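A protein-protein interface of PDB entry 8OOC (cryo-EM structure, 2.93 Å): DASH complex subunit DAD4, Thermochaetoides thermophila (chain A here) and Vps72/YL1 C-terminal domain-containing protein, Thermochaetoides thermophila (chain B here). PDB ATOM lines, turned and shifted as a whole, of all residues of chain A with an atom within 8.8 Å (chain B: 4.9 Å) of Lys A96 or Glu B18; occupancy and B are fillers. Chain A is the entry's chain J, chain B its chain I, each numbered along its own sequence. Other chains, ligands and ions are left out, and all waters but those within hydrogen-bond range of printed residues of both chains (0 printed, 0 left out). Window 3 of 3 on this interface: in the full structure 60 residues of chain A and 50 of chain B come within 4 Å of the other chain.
Hydrophobic or aromatic side chains of chain B within 4 Å of the printed part of chain A: Val B17 and Leu B20. Printed residues of chain A that touch a printed residue of chain B: Tyr A38, Tyr A89, Asp A91, Met A94, Lys A96, Thr A97, Phe A98, Ser A99 and Phe A100. Among the printed residues, 13 pairs touch across the chains. Among the printed residues, Asp or Glu carboxylates within 4 Å of a Lys or Arg side-chain nitrogen of the other chain: Lys A96 with Glu B18.
The side-chain carboxylate of Asp A91 is in hydrogen-bond range of the side-chain amide nitrogen of Gln B14. The side-chain amide oxygen of Gln B14 lies close to the side-chain sulfur of Met A94 (3.4 Å). The side-chain carboxylate (OE1) of Glu B18 lies within salt-bridge range of the side-chain amino group (NZ) of Lys A96. The side-chain carboxylate (OD1) of Asp B21 lies within hydrogen-bond range of the backbone NH (N) of Ser A99, 2.8 Å away. O of Thr A97 sits close to OD2 of Asp B21.
Of chain B, only Glu B18 (2.8 Å) comes within 4 Å of Lys A96. Of chain A, only Lys A96 comes within 4 Å of Glu B18. Of the printed residues of chain B, Phe A98 touches Val B17 (3.5 Å) and Asp B21 (3.5 Å). Of the printed residues of chain A, Leu B20 touches Tyr A38, Ser A99 and Phe A100. Of the printed residues of chain B, Asp A91 touches Gln B14.
Among the printed residues, pairs that only touch across the chains: Tyr A38 with Gln B19, Phe A98 with Asp B21, Phe A100 with Leu B20, Phe A98 with Val B17, Tyr A38 with Leu B20, Tyr A89 with Val B17, Phe A100 with Val B17 and Ser A99 with Leu B20.
OE2 of Glu B18 sits at hydrogen-bond distance from OG of Ser B24 (3.0 Å). The side-chain carboxylate (OD2) of Asp B21 sits at hydrogen-bond distance from the backbone NH (N) of Ser B24, at 3.0 Å. O of Tyr A89 is in hydrogen-bond range of N of Phe A98 (2.8 Å). The side-chain hydroxyl (OG1) of Thr A97 sits close to the guanidinium group (NH1) of Arg A90 (3.5 Å).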
ATOM      1  N   TYR A  38     -36.526 -15.039 -19.365  1.00  0.00           N
ATOM      2  CA  TYR A  38     -35.171 -14.497 -19.397  1.00  0.00           C
ATOM      3  C   TYR A  38     -34.990 -13.368 -18.386  1.00  0.00           C
ATOM      4  O   TYR A  38     -35.897 -12.563 -18.158  1.00  0.00           O
ATOM      5  CB  TYR A  38     -34.857 -14.009 -20.813  1.00  0.00           C
ATOM      6  CG  TYR A  38     -33.467 -13.450 -21.004  1.00  0.00           C
ATOM      7  CD1 TYR A  38     -32.382 -14.294 -21.202  1.00  0.00           C
ATOM      8  CD2 TYR A  38     -33.246 -12.081 -21.031  1.00  0.00           C
ATOM      9  CE1 TYR A  38     -31.110 -13.791 -21.377  1.00  0.00           C
ATOM     10  CE2 TYR A  38     -31.979 -11.569 -21.222  1.00  0.00           C
ATOM     11  CZ  TYR A  38     -30.914 -12.427 -21.389  1.00  0.00           C
ATOM     12  OH  TYR A  38     -29.651 -11.920 -21.590  1.00  0.00           O
ATOM     13  N   LYS A  88     -23.432 -27.367 -23.108  1.00  0.00           N
ATOM     14  CA  LYS A  88     -22.729 -26.917 -24.307  1.00  0.00           C
ATOM     15  C   LYS A  88     -22.893 -27.946 -25.415  1.00  0.00           C
ATOM     16  O   LYS A  88     -22.536 -29.112 -25.231  1.00  0.00           O
ATOM     17  CB  LYS A  88     -21.249 -26.676 -24.004  1.00  0.00           C
ATOM     18  CG  LYS A  88     -20.476 -26.023 -25.133  1.00  0.00           C
ATOM     19  CD  LYS A  88     -19.073 -25.647 -24.684  1.00  0.00           C
ATOM     20  CE  LYS A  88     -18.265 -26.870 -24.288  1.00  0.00           C
ATOM     21  NZ  LYS A  88     -16.856 -26.511 -23.961  1.00  0.00           N
ATOM     22  N   TYR A  89     -23.426 -27.519 -26.561  1.00  0.00           N
ATOM     23  CA  TYR A  89     -23.735 -28.443 -27.644  1.00  0.00           C
ATOM     24  C   TYR A  89     -23.792 -27.662 -28.951  1.00  0.00           C
ATOM     25  O   TYR A  89     -23.857 -26.430 -28.961  1.00  0.00           O
ATOM     26  CB  TYR A  89     -25.050 -29.191 -27.390  1.00  0.00           C
ATOM     27  CG  TYR A  89     -26.291 -28.321 -27.398  1.00  0.00           C
ATOM     28  CD1 TYR A  89     -26.956 -28.034 -28.585  1.00  0.00           C
ATOM     29  CD2 TYR A  89     -26.805 -27.801 -26.220  1.00  0.00           C
ATOM     30  CE1 TYR A  89     -28.077 -27.228 -28.600  1.00  0.00           C
ATOM     31  CE2 TYR A  89     -27.939 -27.009 -26.223  1.00  0.00           C
ATOM     32  CZ  TYR A  89     -28.567 -26.722 -27.416  1.00  0.00           C
ATOM     33  OH  TYR A  89     -29.707 -25.952 -27.422  1.00  0.00           O
ATOM     34  N   ARG A  90     -23.765 -28.403 -30.057  1.00  0.00           N
ATOM     35  CA  ARG A  90     -24.071 -27.877 -31.383  1.00  0.00           C
ATOM     36  C   ARG A  90     -25.350 -28.515 -31.904  1.00  0.00           C
ATOM     37  O   ARG A  90     -25.454 -29.745 -31.959  1.00  0.00           O
ATOM     38  CB  ARG A  90     -22.923 -28.154 -32.356  1.00  0.00           C
ATOM     39  CG  ARG A  90     -21.739 -27.220 -32.210  1.00  0.00           C
ATOM     40  CD  ARG A  90     -20.517 -27.779 -32.922  1.00  0.00           C
ATOM     41  NE  ARG A  90     -19.970 -28.949 -32.243  1.00  0.00           N
ATOM     42  CZ  ARG A  90     -19.279 -28.912 -31.111  1.00  0.00           C
ATOM     43  NH1 ARG A  90     -19.018 -27.770 -30.496  1.00  0.00           N
ATOM     44  NH2 ARG A  90     -18.838 -30.051 -30.585  1.00  0.00           N
ATOM     45  N   ASP A  91     -26.320 -27.686 -32.286  1.00  0.00           N
ATOM     46  CA  ASP A  91     -27.340 -28.107 -33.245  1.00  0.00           C
ATOM     47  C   ASP A  91     -26.720 -28.114 -34.637  1.00  0.00           C
ATOM     48  O   ASP A  91     -26.658 -27.083 -35.308  1.00  0.00           O
ATOM     49  CB  ASP A  91     -28.548 -27.180 -33.182  1.00  0.00           C
ATOM     50  CG  ASP A  91     -29.473 -27.507 -32.027  1.00  0.00           C
ATOM     51  OD1 ASP A  91     -29.275 -28.559 -31.385  1.00  0.00           O
ATOM     52  OD2 ASP A  91     -30.396 -26.709 -31.758  1.00  0.00           O
ATOM     53  N   ARG A  92     -26.243 -29.286 -35.069  1.00  0.00           N
ATOM     54  CA  ARG A  92     -25.303 -29.338 -36.185  1.00  0.00           C
ATOM     55  C   ARG A  92     -25.932 -28.853 -37.487  1.00  0.00           C
ATOM     56  O   ARG A  92     -25.227 -28.344 -38.366  1.00  0.00           O
ATOM     57  CB  ARG A  92     -24.765 -30.759 -36.351  1.00  0.00           C
ATOM     58  CG  ARG A  92     -23.462 -30.843 -37.129  1.00  0.00           C
ATOM     59  CD  ARG A  92     -22.349 -30.088 -36.417  1.00  0.00           C
ATOM     60  NE  ARG A  92     -21.036 -30.395 -36.968  1.00  0.00           N
ATOM     61  CZ  ARG A  92     -20.254 -31.378 -36.540  1.00  0.00           C
ATOM     62  NH1 ARG A  92     -20.633 -32.185 -35.563  1.00  0.00           N
ATOM     63  NH2 ARG A  92     -19.067 -31.559 -37.111  1.00  0.00           N
ATOM     64  N   LYS A  93     -27.253 -29.001 -37.629  1.00  0.00           N
ATOM     65  CA  LYS A  93     -27.967 -28.389 -38.746  1.00  0.00           C
ATOM     66  C   LYS A  93     -27.945 -26.865 -38.685  1.00  0.00           C
ATOM     67  O   LYS A  93     -28.012 -26.207 -39.729  1.00  0.00           O
ATOM     68  CB  LYS A  93     -29.407 -28.900 -38.792  1.00  0.00           C
ATOM     69  CG  LYS A  93     -30.240 -28.561 -37.569  1.00  0.00           C
ATOM     70  CD  LYS A  93     -31.610 -29.213 -37.652  1.00  0.00           C
ATOM     71  CE  LYS A  93     -32.436 -28.930 -36.409  1.00  0.00           C
ATOM     72  NZ  LYS A  93     -33.763 -29.604 -36.469  1.00  0.00           N
ATOM     73  N   MET A  94     -27.852 -26.289 -37.488  1.00  0.00           N
ATOM     74  CA  MET A  94     -27.700 -24.847 -37.354  1.00  0.00           C
ATOM     75  C   MET A  94     -26.243 -24.414 -37.275  1.00  0.00           C
ATOM     76  O   MET A  94     -25.943 -23.241 -37.527  1.00  0.00           O
ATOM     77  CB  MET A  94     -28.456 -24.367 -36.110  1.00  0.00           C
ATOM     78  CG  MET A  94     -28.696 -22.869 -36.032  1.00  0.00           C
ATOM     79  SD  MET A  94     -29.870 -22.454 -34.727  1.00  0.00           S
ATOM     80  CE  MET A  94     -30.031 -20.686 -34.957  1.00  0.00           C
ATOM     81  N   GLY A  95     -25.338 -25.328 -36.944  1.00  0.00           N
ATOM     82  CA  GLY A  95     -23.915 -25.121 -37.130  1.00  0.00           C
ATOM     83  C   GLY A  95     -23.241 -24.364 -36.006  1.00  0.00           C
ATOM     84  O   GLY A  95     -22.155 -24.749 -35.560  1.00  0.00           O
ATOM     85  N   LYS A  96     -23.865 -23.284 -35.544  1.00  0.00           N
ATOM     86  CA  LYS A  96     -23.317 -22.527 -34.427  1.00  0.00           C
ATOM     87  C   LYS A  96     -23.332 -23.367 -33.155  1.00  0.00           C
ATOM     88  O   LYS A  96     -24.242 -24.169 -32.929  1.00  0.00           O
ATOM     89  CB  LYS A  96     -24.090 -21.221 -34.241  1.00  0.00           C
ATOM     90  CG  LYS A  96     -25.590 -21.374 -34.105  1.00  0.00           C
ATOM     91  CD  LYS A  96     -26.226 -20.053 -33.700  1.00  0.00           C
ATOM     92  CE  LYS A  96     -25.866 -18.942 -34.672  1.00  0.00           C
ATOM     93  NZ  LYS A  96     -26.629 -17.694 -34.392  1.00  0.00           N
ATOM     94  N   THR A  97     -22.313 -23.177 -32.323  1.00  0.00           N
ATOM     95  CA  THR A  97     -22.306 -23.718 -30.972  1.00  0.00           C
ATOM     96  C   THR A  97     -23.211 -22.902 -30.053  1.00  0.00           C
ATOM     97  O   THR A  97     -23.337 -21.683 -30.190  1.00  0.00           O
ATOM     98  CB  THR A  97     -20.873 -23.742 -30.427  1.00  0.00           C
ATOM     99  OG1 THR A  97     -20.055 -24.562 -31.272  1.00  0.00           O
ATOM    100  CG2 THR A  97     -20.827 -24.305 -29.014  1.00  0.00           C
ATOM    101  N   PHE A  98     -23.846 -23.595 -29.108  1.00  0.00           N
ATOM    102  CA  PHE A  98     -24.559 -22.969 -28.006  1.00  0.00           C
ATOM    103  C   PHE A  98     -23.984 -23.435 -26.676  1.00  0.00           C
ATOM    104  O   PHE A  98     -23.503 -24.565 -26.548  1.00  0.00           O
ATOM    105  CB  PHE A  98     -26.055 -23.296 -28.040  1.00  0.00           C
ATOM    106  CG  PHE A  98     -26.751 -22.847 -29.289  1.00  0.00           C
ATOM    107  CD1 PHE A  98     -26.946 -21.501 -29.539  1.00  0.00           C
ATOM    108  CD2 PHE A  98     -27.227 -23.771 -30.201  1.00  0.00           C
ATOM    109  CE1 PHE A  98     -27.596 -21.084 -30.681  1.00  0.00           C
ATOM    110  CE2 PHE A  98     -27.878 -23.360 -31.346  1.00  0.00           C
ATOM    111  CZ  PHE A  98     -28.063 -22.016 -31.586  1.00  0.00           C
ATOM    112  N   SER A  99     -24.035 -22.546 -25.687  1.00  0.00           N
ATOM    113  CA  SER A  99     -23.445 -22.799 -24.382  1.00  0.00           C
ATOM    114  C   SER A  99     -24.292 -22.115 -23.321  1.00  0.00           C
ATOM    115  O   SER A  99     -24.835 -21.032 -23.546  1.00  0.00           O
ATOM    116  CB  SER A  99     -21.998 -22.300 -24.306  1.00  0.00           C
ATOM    117  OG  SER A  99     -21.942 -20.894 -24.465  1.00  0.00           O
ATOM    118  N   PHE A 100     -24.383 -22.750 -22.154  1.00  0.00           N
ATOM    119  CA  PHE A 100     -25.345 -22.366 -21.132  1.00  0.00           C
ATOM    120  C   PHE A 100     -24.739 -22.674 -19.773  1.00  0.00           C
ATOM    121  O   PHE A 100     -23.903 -23.572 -19.648  1.00  0.00           O
ATOM    122  CB  PHE A 100     -26.674 -23.115 -21.292  1.00  0.00           C
ATOM    123  CG  PHE A 100     -27.312 -22.954 -22.642  1.00  0.00           C
ATOM    124  CD1 PHE A 100     -27.731 -21.712 -23.085  1.00  0.00           C
ATOM    125  CD2 PHE A 100     -27.491 -24.047 -23.470  1.00  0.00           C
ATOM    126  CE1 PHE A 100     -28.315 -21.567 -24.328  1.00  0.00           C
ATOM    127  CE2 PHE A 100     -28.077 -23.906 -24.713  1.00  0.00           C
ATOM    128  CZ  PHE A 100     -28.490 -22.664 -25.142  1.00  0.00           C
ATOM    129  N   TYR A 106     -32.181 -26.070 -19.603  1.00  0.00           N
ATOM    130  CA  TYR A 106     -33.625 -26.034 -19.399  1.00  0.00           C
ATOM    131  C   TYR A 106     -34.083 -26.786 -18.156  1.00  0.00           C
ATOM    132  O   TYR A 106     -35.248 -26.645 -17.768  1.00  0.00           O
ATOM    133  CB  TYR A 106     -34.332 -26.571 -20.640  1.00  0.00           C
ATOM    134  CG  TYR A 106     -34.588 -25.492 -21.665  1.00  0.00           C
ATOM    135  CD1 TYR A 106     -33.534 -24.839 -22.289  1.00  0.00           C
ATOM    136  CD2 TYR A 106     -35.881 -25.113 -21.996  1.00  0.00           C
ATOM    137  CE1 TYR A 106     -33.760 -23.846 -23.218  1.00  0.00           C
ATOM    138  CE2 TYR A 106     -36.117 -24.121 -22.926  1.00  0.00           C
ATOM    139  CZ  TYR A 106     -35.053 -23.491 -23.534  1.00  0.00           C
ATOM    140  OH  TYR A 106     -35.282 -22.503 -24.464  1.00  0.00           O
ATOM    141  N   GLN B  14     -35.455 -21.325 -31.326  1.00  0.00           N
ATOM    142  CA  GLN B  14     -34.064 -21.071 -31.690  1.00  0.00           C
ATOM    143  C   GLN B  14     -33.649 -19.631 -31.410  1.00  0.00           C
ATOM    144  O   GLN B  14     -32.474 -19.370 -31.126  1.00  0.00           O
ATOM    145  CB  GLN B  14     -33.837 -21.407 -33.166  1.00  0.00           C
ATOM    146  CG  GLN B  14     -33.933 -22.893 -33.510  1.00  0.00           C
ATOM    147  CD  GLN B  14     -32.835 -23.742 -32.883  1.00  0.00           C
ATOM    148  OE1 GLN B  14     -31.943 -23.235 -32.203  1.00  0.00           O
ATOM    149  NE2 GLN B  14     -32.902 -25.048 -33.113  1.00  0.00           N
ATOM    150  N   ALA B  15     -34.588 -18.685 -31.490  1.00  0.00           N
ATOM    151  CA  ALA B  15     -34.306 -17.320 -31.051  1.00  0.00           C
ATOM    152  C   ALA B  15     -34.024 -17.253 -29.554  1.00  0.00           C
ATOM    153  O   ALA B  15     -33.158 -16.490 -29.113  1.00  0.00           O
ATOM    154  CB  ALA B  15     -35.471 -16.403 -31.418  1.00  0.00           C
ATOM    155  N   LEU B  16     -34.746 -18.042 -28.757  1.00  0.00           N
ATOM    156  CA  LEU B  16     -34.426 -18.158 -27.336  1.00  0.00           C
ATOM    157  C   LEU B  16     -33.082 -18.843 -27.112  1.00  0.00           C
ATOM    158  O   LEU B  16     -32.285 -18.397 -26.279  1.00  0.00           O
ATOM    159  CB  LEU B  16     -35.538 -18.915 -26.610  1.00  0.00           C
ATOM    160  CG  LEU B  16     -36.623 -18.080 -25.925  1.00  0.00           C
ATOM    161  CD1 LEU B  16     -36.048 -17.318 -24.744  1.00  0.00           C
ATOM    162  CD2 LEU B  16     -37.295 -17.130 -26.906  1.00  0.00           C
ATOM    163  N   VAL B  17     -32.821 -19.933 -27.835  1.00  0.00           N
ATOM    164  CA  VAL B  17     -31.535 -20.623 -27.736  1.00  0.00           C
ATOM    165  C   VAL B  17     -30.385 -19.688 -28.092  1.00  0.00           C
ATOM    166  O   VAL B  17     -29.321 -19.717 -27.462  1.00  0.00           O
ATOM    167  CB  VAL B  17     -31.543 -21.883 -28.622  1.00  0.00           C
ATOM    168  CG1 VAL B  17     -30.177 -22.543 -28.628  1.00  0.00           C
ATOM    169  CG2 VAL B  17     -32.604 -22.862 -28.143  1.00  0.00           C
ATOM    170  N   GLU B  18     -30.583 -18.835 -29.099  1.00  0.00           N
ATOM    171  CA  GLU B  18     -29.622 -17.773 -29.390  1.00  0.00           C
ATOM    172  C   GLU B  18     -29.535 -16.765 -28.249  1.00  0.00           C
ATOM    173  O   GLU B  18     -28.438 -16.434 -27.782  1.00  0.00           O
ATOM    174  CB  GLU B  18     -30.004 -17.077 -30.696  1.00  0.00           C
ATOM    175  CG  GLU B  18     -29.214 -15.813 -30.995  1.00  0.00           C
ATOM    176  CD  GLU B  18     -27.724 -16.062 -31.091  1.00  0.00           C
ATOM    177  OE1 GLU B  18     -27.322 -17.012 -31.795  1.00  0.00           O
ATOM    178  OE2 GLU B  18     -26.956 -15.302 -30.467  1.00  0.00           O
ATOM    179  N   GLN B  19     -30.684 -16.257 -27.798  1.00  0.00           N
ATOM    180  CA  GLN B  19     -30.717 -15.225 -26.764  1.00  0.00           C
ATOM    181  C   GLN B  19     -30.003 -15.652 -25.484  1.00  0.00           C
ATOM    182  O   GLN B  19     -29.424 -14.810 -24.787  1.00  0.00           O
ATOM    183  CB  GLN B  19     -32.174 -14.862 -26.466  1.00  0.00           C
ATOM    184  CG  GLN B  19     -32.387 -13.949 -25.274  1.00  0.00           C
ATOM    185  CD  GLN B  19     -33.823 -13.475 -25.164  1.00  0.00           C
ATOM    186  OE1 GLN B  19     -34.652 -13.767 -26.025  1.00  0.00           O
ATOM    187  NE2 GLN B  19     -34.124 -12.738 -24.103  1.00  0.00           N
ATOM    188  N   LEU B  20     -30.013 -16.943 -25.166  1.00  0.00           N
ATOM    189  CA  LEU B  20     -29.373 -17.466 -23.965  1.00  0.00           C
ATOM    190  C   LEU B  20     -27.887 -17.777 -24.125  1.00  0.00           C
ATOM    191  O   LEU B  20     -27.214 -18.000 -23.112  1.00  0.00           O
ATOM    192  CB  LEU B  20     -30.102 -18.724 -23.487  1.00  0.00           C
ATOM    193  CG  LEU B  20     -31.525 -18.504 -22.971  1.00  0.00           C
ATOM    194  CD1 LEU B  20     -32.270 -19.824 -22.868  1.00  0.00           C
ATOM    195  CD2 LEU B  20     -31.499 -17.792 -21.632  1.00  0.00           C
ATOM    196  N   ASP B  21     -27.355 -17.805 -25.345  1.00  0.00           N
ATOM    197  CA  ASP B  21     -26.052 -18.420 -25.580  1.00  0.00           C
ATOM    198  C   ASP B  21     -24.926 -17.574 -24.989  1.00  0.00           C
ATOM    199  O   ASP B  21     -24.776 -16.393 -25.320  1.00  0.00           O
ATOM    200  CB  ASP B  21     -25.837 -18.620 -27.079  1.00  0.00           C
ATOM    201  CG  ASP B  21     -24.444 -19.118 -27.407  1.00  0.00           C
ATOM    202  OD1 ASP B  21     -23.879 -19.888 -26.602  1.00  0.00           O
ATOM    203  OD2 ASP B  21     -23.912 -18.740 -28.473  1.00  0.00           O
ATOM    204  N   SER B  24     -22.541 -16.178 -27.658  1.00  0.00           N
ATOM    205  CA  SER B  24     -22.969 -14.916 -28.251  1.00  0.00           C
ATOM    206  C   SER B  24     -22.589 -13.735 -27.365  1.00  0.00           C
ATOM    207  O   SER B  24     -22.152 -12.692 -27.864  1.00  0.00           O
ATOM    208  CB  SER B  24     -24.475 -14.939 -28.499  1.00  0.00           C
ATOM    209  OG  SER B  24     -24.924 -13.701 -29.022  1.00  0.00           O
